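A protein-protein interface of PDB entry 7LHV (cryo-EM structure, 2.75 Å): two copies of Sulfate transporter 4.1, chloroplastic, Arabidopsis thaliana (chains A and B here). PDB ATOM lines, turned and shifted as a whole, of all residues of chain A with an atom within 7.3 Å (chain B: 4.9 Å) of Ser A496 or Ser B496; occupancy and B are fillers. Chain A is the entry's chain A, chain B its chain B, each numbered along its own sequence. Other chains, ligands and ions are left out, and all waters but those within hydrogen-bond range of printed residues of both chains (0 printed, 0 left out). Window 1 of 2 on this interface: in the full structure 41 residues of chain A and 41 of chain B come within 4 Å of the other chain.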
ATOM      1  N   PHE A 203      -6.540 -12.658  26.935  1.00  0.00           N
ATOM      2  CA  PHE A 203      -6.476 -13.956  26.279  1.00  0.00           C
ATOM      3  C   PHE A 203      -5.049 -14.410  26.014  1.00  0.00           C
ATOM      4  O   PHE A 203      -4.846 -15.569  25.642  1.00  0.00           O
ATOM      5  CB  PHE A 203      -7.262 -13.929  24.963  1.00  0.00           C
ATOM      6  CG  PHE A 203      -6.561 -13.201  23.851  1.00  0.00           C
ATOM      7  CD1 PHE A 203      -6.730 -11.841  23.682  1.00  0.00           C
ATOM      8  CD2 PHE A 203      -5.734 -13.878  22.971  1.00  0.00           C
ATOM      9  CE1 PHE A 203      -6.088 -11.170  22.666  1.00  0.00           C
ATOM     10  CE2 PHE A 203      -5.089 -13.210  21.959  1.00  0.00           C
ATOM     11  CZ  PHE A 203      -5.267 -11.855  21.804  1.00  0.00           C
ATOM     12  N   ALA A 490      -4.020 -17.490  17.369  1.00  0.00           N
ATOM     13  CA  ALA A 490      -4.158 -18.707  16.582  1.00  0.00           C
ATOM     14  C   ALA A 490      -4.635 -19.860  17.446  1.00  0.00           C
ATOM     15  O   ALA A 490      -5.495 -20.641  17.030  1.00  0.00           O
ATOM     16  CB  ALA A 490      -2.832 -19.054  15.911  1.00  0.00           C
ATOM     17  N   PHE A 491      -4.100 -19.978  18.661  1.00  0.00           N
ATOM     18  CA  PHE A 491      -4.510 -21.079  19.527  1.00  0.00           C
ATOM     19  C   PHE A 491      -5.918 -20.867  20.073  1.00  0.00           C
ATOM     20  O   PHE A 491      -6.680 -21.830  20.229  1.00  0.00           O
ATOM     21  CB  PHE A 491      -3.493 -21.260  20.647  1.00  0.00           C
ATOM     22  CG  PHE A 491      -2.329 -22.115  20.251  1.00  0.00           C
ATOM     23  CD1 PHE A 491      -2.496 -23.466  20.018  1.00  0.00           C
ATOM     24  CD2 PHE A 491      -1.076 -21.561  20.074  1.00  0.00           C
ATOM     25  CE1 PHE A 491      -1.431 -24.250  19.637  1.00  0.00           C
ATOM     26  CE2 PHE A 491      -0.009 -22.341  19.693  1.00  0.00           C
ATOM     27  CZ  PHE A 491      -0.186 -23.687  19.476  1.00  0.00           C
ATOM     28  N   VAL A 492      -6.296 -19.615  20.347  1.00  0.00           N
ATOM     29  CA  VAL A 492      -7.672 -19.331  20.753  1.00  0.00           C
ATOM     30  C   VAL A 492      -8.641 -19.707  19.639  1.00  0.00           C
ATOM     31  O   VAL A 492      -9.682 -20.331  19.883  1.00  0.00           O
ATOM     32  CB  VAL A 492      -7.815 -17.849  21.149  1.00  0.00           C
ATOM     33  CG1 VAL A 492      -9.271 -17.431  21.125  1.00  0.00           C
ATOM     34  CG2 VAL A 492      -7.220 -17.611  22.518  1.00  0.00           C
ATOM     35  N   ILE A 493      -8.310 -19.343  18.401  1.00  0.00           N
ATOM     36  CA  ILE A 493      -9.171 -19.652  17.265  1.00  0.00           C
ATOM     37  C   ILE A 493      -9.227 -21.156  17.027  1.00  0.00           C
ATOM     38  O   ILE A 493     -10.284 -21.705  16.705  1.00  0.00           O
ATOM     39  CB  ILE A 493      -8.690 -18.890  16.017  1.00  0.00           C
ATOM     40  CG1 ILE A 493      -8.974 -17.397  16.176  1.00  0.00           C
ATOM     41  CG2 ILE A 493      -9.356 -19.426  14.768  1.00  0.00           C
ATOM     42  CD1 ILE A 493      -8.260 -16.538  15.174  1.00  0.00           C
ATOM     43  N   HIS A 494      -8.095 -21.845  17.180  1.00  0.00           N
ATOM     44  CA  HIS A 494      -8.088 -23.294  17.023  1.00  0.00           C
ATOM     45  C   HIS A 494      -8.963 -23.968  18.069  1.00  0.00           C
ATOM     46  O   HIS A 494      -9.679 -24.926  17.763  1.00  0.00           O
ATOM     47  CB  HIS A 494      -6.659 -23.825  17.103  1.00  0.00           C
ATOM     48  CG  HIS A 494      -6.560 -25.307  16.920  1.00  0.00           C
ATOM     49  ND1 HIS A 494      -6.544 -26.187  17.981  1.00  0.00           N
ATOM     50  CD2 HIS A 494      -6.466 -26.063  15.802  1.00  0.00           C
ATOM     51  CE1 HIS A 494      -6.447 -27.421  17.523  1.00  0.00           C
ATOM     52  NE2 HIS A 494      -6.397 -27.375  16.206  1.00  0.00           N
ATOM     53  N   GLU A 495      -8.907 -23.496  19.315  1.00  0.00           N
ATOM     54  CA  GLU A 495      -9.766 -24.071  20.346  1.00  0.00           C
ATOM     55  C   GLU A 495     -11.234 -23.785  20.067  1.00  0.00           C
ATOM     56  O   GLU A 495     -12.086 -24.664  20.247  1.00  0.00           O
ATOM     57  CB  GLU A 495      -9.374 -23.541  21.721  1.00  0.00           C
ATOM     58  CG  GLU A 495     -10.202 -24.129  22.847  1.00  0.00           C
ATOM     59  CD  GLU A 495      -9.978 -25.619  23.012  1.00  0.00           C
ATOM     60  OE1 GLU A 495      -8.888 -26.102  22.643  1.00  0.00           O
ATOM     61  OE2 GLU A 495     -10.894 -26.309  23.504  1.00  0.00           O
ATOM     62  N   SER A 496     -11.555 -22.565  19.635  1.00  0.00           N
ATOM     63  CA  SER A 496     -12.948 -22.222  19.367  1.00  0.00           C
ATOM     64  C   SER A 496     -13.497 -23.008  18.184  1.00  0.00           C
ATOM     65  O   SER A 496     -14.670 -23.392  18.178  1.00  0.00           O
ATOM     66  CB  SER A 496     -13.085 -20.721  19.121  1.00  0.00           C
ATOM     67  OG  SER A 496     -12.785 -19.981  20.291  1.00  0.00           O
ATOM     68  N   ALA A 497     -12.663 -23.262  17.181  1.00  0.00           N
ATOM     69  CA  ALA A 497     -13.093 -23.871  15.932  1.00  0.00           C
ATOM     70  C   ALA A 497     -13.118 -25.391  15.967  1.00  0.00           C
ATOM     71  O   ALA A 497     -13.477 -26.009  14.961  1.00  0.00           O
ATOM     72  CB  ALA A 497     -12.188 -23.407  14.788  1.00  0.00           C
ATOM     73  N   ASN A 498     -12.749 -26.018  17.081  1.00  0.00           N
ATOM     74  CA  ASN A 498     -12.760 -27.476  17.202  1.00  0.00           C
ATOM     75  C   ASN A 498     -13.488 -27.881  18.476  1.00  0.00           C
ATOM     76  O   ASN A 498     -12.873 -28.382  19.424  1.00  0.00           O
ATOM     77  CB  ASN A 498     -11.338 -28.036  17.186  1.00  0.00           C
ATOM     78  CG  ASN A 498     -10.646 -27.824  15.860  1.00  0.00           C
ATOM     79  OD1 ASN A 498     -11.268 -27.891  14.802  1.00  0.00           O
ATOM     80  ND2 ASN A 498      -9.346 -27.568  15.908  1.00  0.00           N
ATOM     81  N   PRO A 499     -14.803 -27.690  18.528  1.00  0.00           N
ATOM     82  CA  PRO A 499     -15.557 -28.100  19.713  1.00  0.00           C
ATOM     83  C   PRO A 499     -15.647 -29.613  19.818  1.00  0.00           C
ATOM     84  O   PRO A 499     -15.533 -30.347  18.835  1.00  0.00           O
ATOM     85  CB  PRO A 499     -16.936 -27.479  19.487  1.00  0.00           C
ATOM     86  CG  PRO A 499     -17.060 -27.414  18.018  1.00  0.00           C
ATOM     87  CD  PRO A 499     -15.684 -27.112  17.499  1.00  0.00           C
ATOM     88  N   SER A 535     -20.807 -27.721  23.643  1.00  0.00           N
ATOM     89  CA  SER A 535     -20.425 -26.316  23.573  1.00  0.00           C
ATOM     90  C   SER A 535     -21.567 -25.485  23.008  1.00  0.00           C
ATOM     91  O   SER A 535     -22.423 -26.018  22.291  1.00  0.00           O
ATOM     92  CB  SER A 535     -19.180 -26.132  22.707  1.00  0.00           C
ATOM     93  OG  SER A 535     -19.333 -26.790  21.463  1.00  0.00           O
ATOM     94  N   PRO A 536     -21.626 -24.189  23.308  1.00  0.00           N
ATOM     95  CA  PRO A 536     -22.558 -23.319  22.589  1.00  0.00           C
ATOM     96  C   PRO A 536     -22.180 -23.230  21.120  1.00  0.00           C
ATOM     97  O   PRO A 536     -21.003 -23.269  20.756  1.00  0.00           O
ATOM     98  CB  PRO A 536     -22.397 -21.967  23.292  1.00  0.00           C
ATOM     99  CG  PRO A 536     -21.062 -22.032  23.930  1.00  0.00           C
ATOM    100  CD  PRO A 536     -20.870 -23.455  24.333  1.00  0.00           C
ATOM    101  N   TYR A 538     -22.045 -21.110  17.730  1.00  0.00           N
ATOM    102  CA  TYR A 538     -22.022 -19.754  17.203  1.00  0.00           C
ATOM    103  C   TYR A 538     -21.172 -19.757  15.938  1.00  0.00           C
ATOM    104  O   TYR A 538     -20.771 -20.816  15.447  1.00  0.00           O
ATOM    105  CB  TYR A 538     -21.538 -18.760  18.270  1.00  0.00           C
ATOM    106  CG  TYR A 538     -20.103 -18.918  18.718  1.00  0.00           C
ATOM    107  CD1 TYR A 538     -19.678 -20.062  19.372  1.00  0.00           C
ATOM    108  CD2 TYR A 538     -19.181 -17.905  18.517  1.00  0.00           C
ATOM    109  CE1 TYR A 538     -18.376 -20.206  19.787  1.00  0.00           C
ATOM    110  CE2 TYR A 538     -17.877 -18.036  18.933  1.00  0.00           C
ATOM    111  CZ  TYR A 538     -17.480 -19.190  19.566  1.00  0.00           C
ATOM    112  OH  TYR A 538     -16.180 -19.330  19.983  1.00  0.00           O
ATOM    113  N   ALA A 540     -18.196 -19.148  15.089  1.00  0.00           N
ATOM    114  CA  ALA A 540     -16.817 -19.622  15.021  1.00  0.00           C
ATOM    115  C   ALA A 540     -16.747 -21.132  14.824  1.00  0.00           C
ATOM    116  O   ALA A 540     -15.930 -21.619  14.035  1.00  0.00           O
ATOM    117  CB  ALA A 540     -16.053 -19.211  16.277  1.00  0.00           C
ATOM    118  N   ASN A 541     -17.582 -21.892  15.528  1.00  0.00           N
ATOM    119  CA  ASN A 541     -17.501 -23.346  15.490  1.00  0.00           C
ATOM    120  C   ASN A 541     -18.591 -23.984  14.640  1.00  0.00           C
ATOM    121  O   ASN A 541     -18.774 -25.201  14.706  1.00  0.00           O
ATOM    122  CB  ASN A 541     -17.547 -23.921  16.906  1.00  0.00           C
ATOM    123  CG  ASN A 541     -18.721 -23.411  17.709  1.00  0.00           C
ATOM    124  OD1 ASN A 541     -19.678 -22.871  17.161  1.00  0.00           O
ATOM    125  ND2 ASN A 541     -18.654 -23.581  19.021  1.00  0.00           N
ATOM    126  N   ILE A 542     -19.323 -23.197  13.852  1.00  0.00           N
ATOM    127  CA  ILE A 542     -20.419 -23.765  13.075  1.00  0.00           C
ATOM    128  C   ILE A 542     -19.902 -24.613  11.919  1.00  0.00           C
ATOM    129  O   ILE A 542     -20.544 -25.596  11.530  1.00  0.00           O
ATOM    130  CB  ILE A 542     -21.371 -22.656  12.595  1.00  0.00           C
ATOM    131  CG1 ILE A 542     -22.668 -23.271  12.084  1.00  0.00           C
ATOM    132  CG2 ILE A 542     -20.719 -21.801  11.526  1.00  0.00           C
ATOM    133  CD1 ILE A 542     -23.269 -24.279  13.030  1.00  0.00           C
ATOM    134  N   TYR A 544     -17.127 -26.544  11.810  1.00  0.00           N
ATOM    135  CA  TYR A 544     -16.725 -27.855  12.307  1.00  0.00           C
ATOM    136  C   TYR A 544     -17.940 -28.719  12.615  1.00  0.00           C
ATOM    137  O   TYR A 544     -17.951 -29.918  12.316  1.00  0.00           O
ATOM    138  CB  TYR A 544     -15.848 -27.699  13.548  1.00  0.00           C
ATOM    139  CG  TYR A 544     -15.374 -29.005  14.143  1.00  0.00           C
ATOM    140  CD1 TYR A 544     -14.226 -29.629  13.679  1.00  0.00           C
ATOM    141  CD2 TYR A 544     -16.074 -29.614  15.174  1.00  0.00           C
ATOM    142  CE1 TYR A 544     -13.793 -30.821  14.223  1.00  0.00           C
ATOM    143  CE2 TYR A 544     -15.649 -30.802  15.724  1.00  0.00           C
ATOM    144  CZ  TYR A 544     -14.511 -31.402  15.246  1.00  0.00           C
ATOM    145  OH  TYR A 544     -14.088 -32.589  15.797  1.00  0.00           O
ATOM    146  N   VAL B 492     -15.290 -13.575  19.202  1.00  0.00           N
ATOM    147  CA  VAL B 492     -14.685 -14.875  19.488  1.00  0.00           C
ATOM    148  C   VAL B 492     -13.978 -14.845  20.837  1.00  0.00           C
ATOM    149  O   VAL B 492     -14.112 -15.771  21.649  1.00  0.00           O
ATOM    150  CB  VAL B 492     -13.720 -15.274  18.355  1.00  0.00           C
ATOM    151  CG1 VAL B 492     -12.762 -16.349  18.825  1.00  0.00           C
ATOM    152  CG2 VAL B 492     -14.496 -15.750  17.147  1.00  0.00           C
ATOM    153  N   ILE B 493     -13.224 -13.779  21.101  1.00  0.00           N
ATOM    154  CA  ILE B 493     -12.503 -13.654  22.364  1.00  0.00           C
ATOM    155  C   ILE B 493     -13.477 -13.508  23.526  1.00  0.00           C
ATOM    156  O   ILE B 493     -13.261 -14.070  24.604  1.00  0.00           O
ATOM    157  CB  ILE B 493     -11.515 -12.477  22.291  1.00  0.00           C
ATOM    158  CG1 ILE B 493     -10.360 -12.823  21.351  1.00  0.00           C
ATOM    159  CG2 ILE B 493     -10.989 -12.128  23.667  1.00  0.00           C
ATOM    160  CD1 ILE B 493      -9.525 -11.639  20.961  1.00  0.00           C
ATOM    161  N   HIS B 494     -14.561 -12.756  23.330  1.00  0.00           N
ATOM    162  CA  HIS B 494     -15.562 -12.618  24.379  1.00  0.00           C
ATOM    163  C   HIS B 494     -16.212 -13.955  24.703  1.00  0.00           C
ATOM    164  O   HIS B 494     -16.457 -14.266  25.872  1.00  0.00           O
ATOM    165  CB  HIS B 494     -16.621 -11.599  23.967  1.00  0.00           C
ATOM    166  CG  HIS B 494     -17.674 -11.375  25.006  1.00  0.00           C
ATOM    167  ND1 HIS B 494     -18.872 -12.055  25.008  1.00  0.00           N
ATOM    168  CD2 HIS B 494     -17.711 -10.544  26.073  1.00  0.00           C
ATOM    169  CE1 HIS B 494     -19.601 -11.654  26.033  1.00  0.00           C
ATOM    170  NE2 HIS B 494     -18.921 -10.738  26.695  1.00  0.00           N
ATOM    171  N   GLU B 495     -16.517 -14.755  23.680  1.00  0.00           N
ATOM    172  CA  GLU B 495     -17.092 -16.071  23.937  1.00  0.00           C
ATOM    173  C   GLU B 495     -16.098 -16.984  24.641  1.00  0.00           C
ATOM    174  O   GLU B 495     -16.471 -17.720  25.562  1.00  0.00           O
ATOM    175  CB  GLU B 495     -17.565 -16.709  22.634  1.00  0.00           C
ATOM    176  CG  GLU B 495     -18.212 -18.066  22.832  1.00  0.00           C
ATOM    177  CD  GLU B 495     -19.501 -17.981  23.624  1.00  0.00           C
ATOM    178  OE1 GLU B 495     -20.149 -16.915  23.596  1.00  0.00           O
ATOM    179  OE2 GLU B 495     -19.865 -18.978  24.281  1.00  0.00           O
ATOM    180  N   SER B 496     -14.831 -16.956  24.224  1.00  0.00           N
ATOM    181  CA  SER B 496     -13.833 -17.820  24.846  1.00  0.00           C
ATOM    182  C   SER B 496     -13.579 -17.423  26.295  1.00  0.00           C
ATOM    183  O   SER B 496     -13.351 -18.284  27.149  1.00  0.00           O
ATOM    184  CB  SER B 496     -12.532 -17.786  24.048  1.00  0.00           C
ATOM    185  OG  SER B 496     -12.705 -18.358  22.764  1.00  0.00           O
ATOM    186  N   ALA B 497     -13.624 -16.128  26.589  1.00  0.00           N
ATOM    187  CA  ALA B 497     -13.257 -15.602  27.895  1.00  0.00           C
ATOM    188  C   ALA B 497     -14.395 -15.616  28.903  1.00  0.00           C
ATOM    189  O   ALA B 497     -14.188 -15.198  30.046  1.00  0.00           O
ATOM    190  CB  ALA B 497     -12.727 -14.173  27.750  1.00  0.00           C
ATOM    191  N   ASN B 498     -15.586 -16.074  28.528  1.00  0.00           N
ATOM    192  CA  ASN B 498     -16.727 -16.135  29.442  1.00  0.00           C
ATOM    193  C   ASN B 498     -17.357 -17.520  29.386  1.00  0.00           C
ATOM    194  O   ASN B 498     -18.477 -17.686  28.892  1.00  0.00           O
ATOM    195  CB  ASN B 498     -17.755 -15.056  29.104  1.00  0.00           C
ATOM    196  CG  ASN B 498     -17.228 -13.659  29.335  1.00  0.00           C
ATOM    197  OD1 ASN B 498     -16.471 -13.414  30.272  1.00  0.00           O
ATOM    198  ND2 ASN B 498     -17.629 -12.730  28.480  1.00  0.00           N
ATOM    199  N   PRO B 499     -16.667 -18.537  29.896  1.00  0.00           N
ATOM    200  CA  PRO B 499     -17.244 -19.881  29.906  1.00  0.00           C
ATOM    201  C   PRO B 499     -18.384 -19.990  30.905  1.00  0.00           C
ATOM    202  O   PRO B 499     -18.481 -19.235  31.873  1.00  0.00           O
ATOM    203  CB  PRO B 499     -16.066 -20.768  30.312  1.00  0.00           C
ATOM    204  CG  PRO B 499     -15.220 -19.880  31.133  1.00  0.00           C
ATOM    205  CD  PRO B 499     -15.332 -18.515  30.517  1.00  0.00           C
ATOM    206  N   TYR B 538      -8.211 -23.515  29.604  1.00  0.00           N
ATOM    207  CA  TYR B 538      -6.945 -23.171  28.973  1.00  0.00           C
ATOM    208  C   TYR B 538      -6.677 -21.694  29.236  1.00  0.00           C
ATOM    209  O   TYR B 538      -7.392 -21.048  30.007  1.00  0.00           O
ATOM    210  CB  TYR B 538      -6.957 -23.543  27.483  1.00  0.00           C
ATOM    211  CG  TYR B 538      -7.928 -22.772  26.618  1.00  0.00           C
ATOM    212  CD1 TYR B 538      -9.295 -22.871  26.811  1.00  0.00           C
ATOM    213  CD2 TYR B 538      -7.474 -21.970  25.583  1.00  0.00           C
ATOM    214  CE1 TYR B 538     -10.180 -22.177  26.020  1.00  0.00           C
ATOM    215  CE2 TYR B 538      -8.351 -21.276  24.784  1.00  0.00           C
ATOM    216  CZ  TYR B 538      -9.702 -21.381  25.009  1.00  0.00           C
ATOM    217  OH  TYR B 538     -10.586 -20.690  24.216  1.00  0.00           O
ATOM    218  N   ALA B 540      -7.092 -18.924  27.784  1.00  0.00           N
ATOM    219  CA  ALA B 540      -8.011 -17.844  27.439  1.00  0.00           C
ATOM    220  C   ALA B 540      -9.065 -17.632  28.520  1.00  0.00           C
ATOM    221  O   ALA B 540      -9.384 -16.488  28.862  1.00  0.00           O
ATOM    222  CB  ALA B 540      -8.675 -18.123  26.093  1.00  0.00           C
ATOM    223  N   ASN B 541      -9.623 -18.709  29.067  1.00  0.00           N
ATOM    224  CA  ASN B 541     -10.721 -18.596  30.018  1.00  0.00           C
ATOM    225  C   ASN B 541     -10.290 -18.827  31.459  1.00  0.00           C
ATOM    226  O   ASN B 541     -11.148 -18.984  32.329  1.00  0.00           O
ATOM    227  CB  ASN B 541     -11.846 -19.565  29.653  1.00  0.00           C
ATOM    228  CG  ASN B 541     -11.361 -20.985  29.469  1.00  0.00           C
ATOM    229  OD1 ASN B 541     -10.265 -21.340  29.892  1.00  0.00           O
ATOM    230  ND2 ASN B 541     -12.182 -21.808  28.833  1.00  0.00           N
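OG of Ser A496 lies within hydrogen-bond range of OG of Ser B496 (3.0 Å).
OH of Tyr A538 sits at hydrogen-bond distance from OG of Ser A496 (3.5 Å). The side-chain amide nitrogen (ND2) of Asn A541 is in hydrogen-bond range of the backbone carbonyl oxygen (O) of Pro A536. OD1 of Asn A541 sits close to O of Tyr A538. The backbone carbonyl oxygen (O) of Val B492 is in hydrogen-bond range of the side-chain hydroxyl (OG) of Ser B496, 3.1 Å away. OG of Ser B496 is in hydrogen-bond range of OH of Tyr B538 (3.5 Å). The backbone carbonyl oxygen (O) of Tyr B538 lies close to the side-chain amide oxygen (OD1) of Asn B541 (2.9 Å).
CE1 of Phe A203 touches CD1 of Ile B493, at 3.9 Å. CG1 of Val A492 touches OG of Ser B496, at 3.9 Å. CG2 of Val A492 touches CB of Ala B540, at 3.9 Å. CG of Glu A495 touches CZ of Tyr B538, 3.5 Å away. Ser A496 touches Val B492. CG of Pro A536 touches OE2 of Glu B495, 3.3 Å away. Tyr A538 touches Glu B495 (CZ to CG, 3.5 Å). CG2 of Val B492 touches CB of Ala A540, 3.9 Å away.
Ser A496 touches just these residues of chain B: Val B492 (3.9 Å) and Ser B496 (3.0 Å). Of the printed residues of chain A, Ser B496 touches Val A492 and Ser A496. Of the printed residues of chain A, Ile B493 touches Phe A203. Printed residues of chain A within 4 Å of Tyr B538: Glu A495. Of the printed residues of chain A, Ala B540 touches Val A492. Of the printed residues of chain B, Glu A495 touches Tyr B538. Of the printed residues of chain B, Pro A536 touches Glu B495 (3.3 Å). Ser A535 touches none of the printed residues of chain B. The nearest printed residue of chain A that does not touch Ala B540 is Phe A203 (4.3 Å).
Of the 18 printed residues of chain A, 7 touch a printed residue of chain B. Printed residues of chain A that touch a printed residue of chain B: Phe A203, Val A492, Glu A495, Ser A496, Pro A536, Tyr A538 and Ala A540. Printed residues of chain B that touch a printed residue of chain A: Val B492, Ile B493, Glu B495, Ser B496, Tyr B538 and Ala B540. Hydrophobic or aromatic side chains of chain B that line the printed part of chain A: Val B492, Ile B493, Tyr B538 and Ala B540. Among the printed residues, 9 pairs touch across the chains.
Val A492 touches Ser B496, and with the chains exchanged Ser A496 touches Val B492. Val A492 touches Ala B540, and with the chains exchanged Ala A540 touches Val B492. Glu A495 touches Tyr B538, and with the chains exchanged Tyr A538 touches Glu B495. Ser B496 touches its own counterpart, Ser A496.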
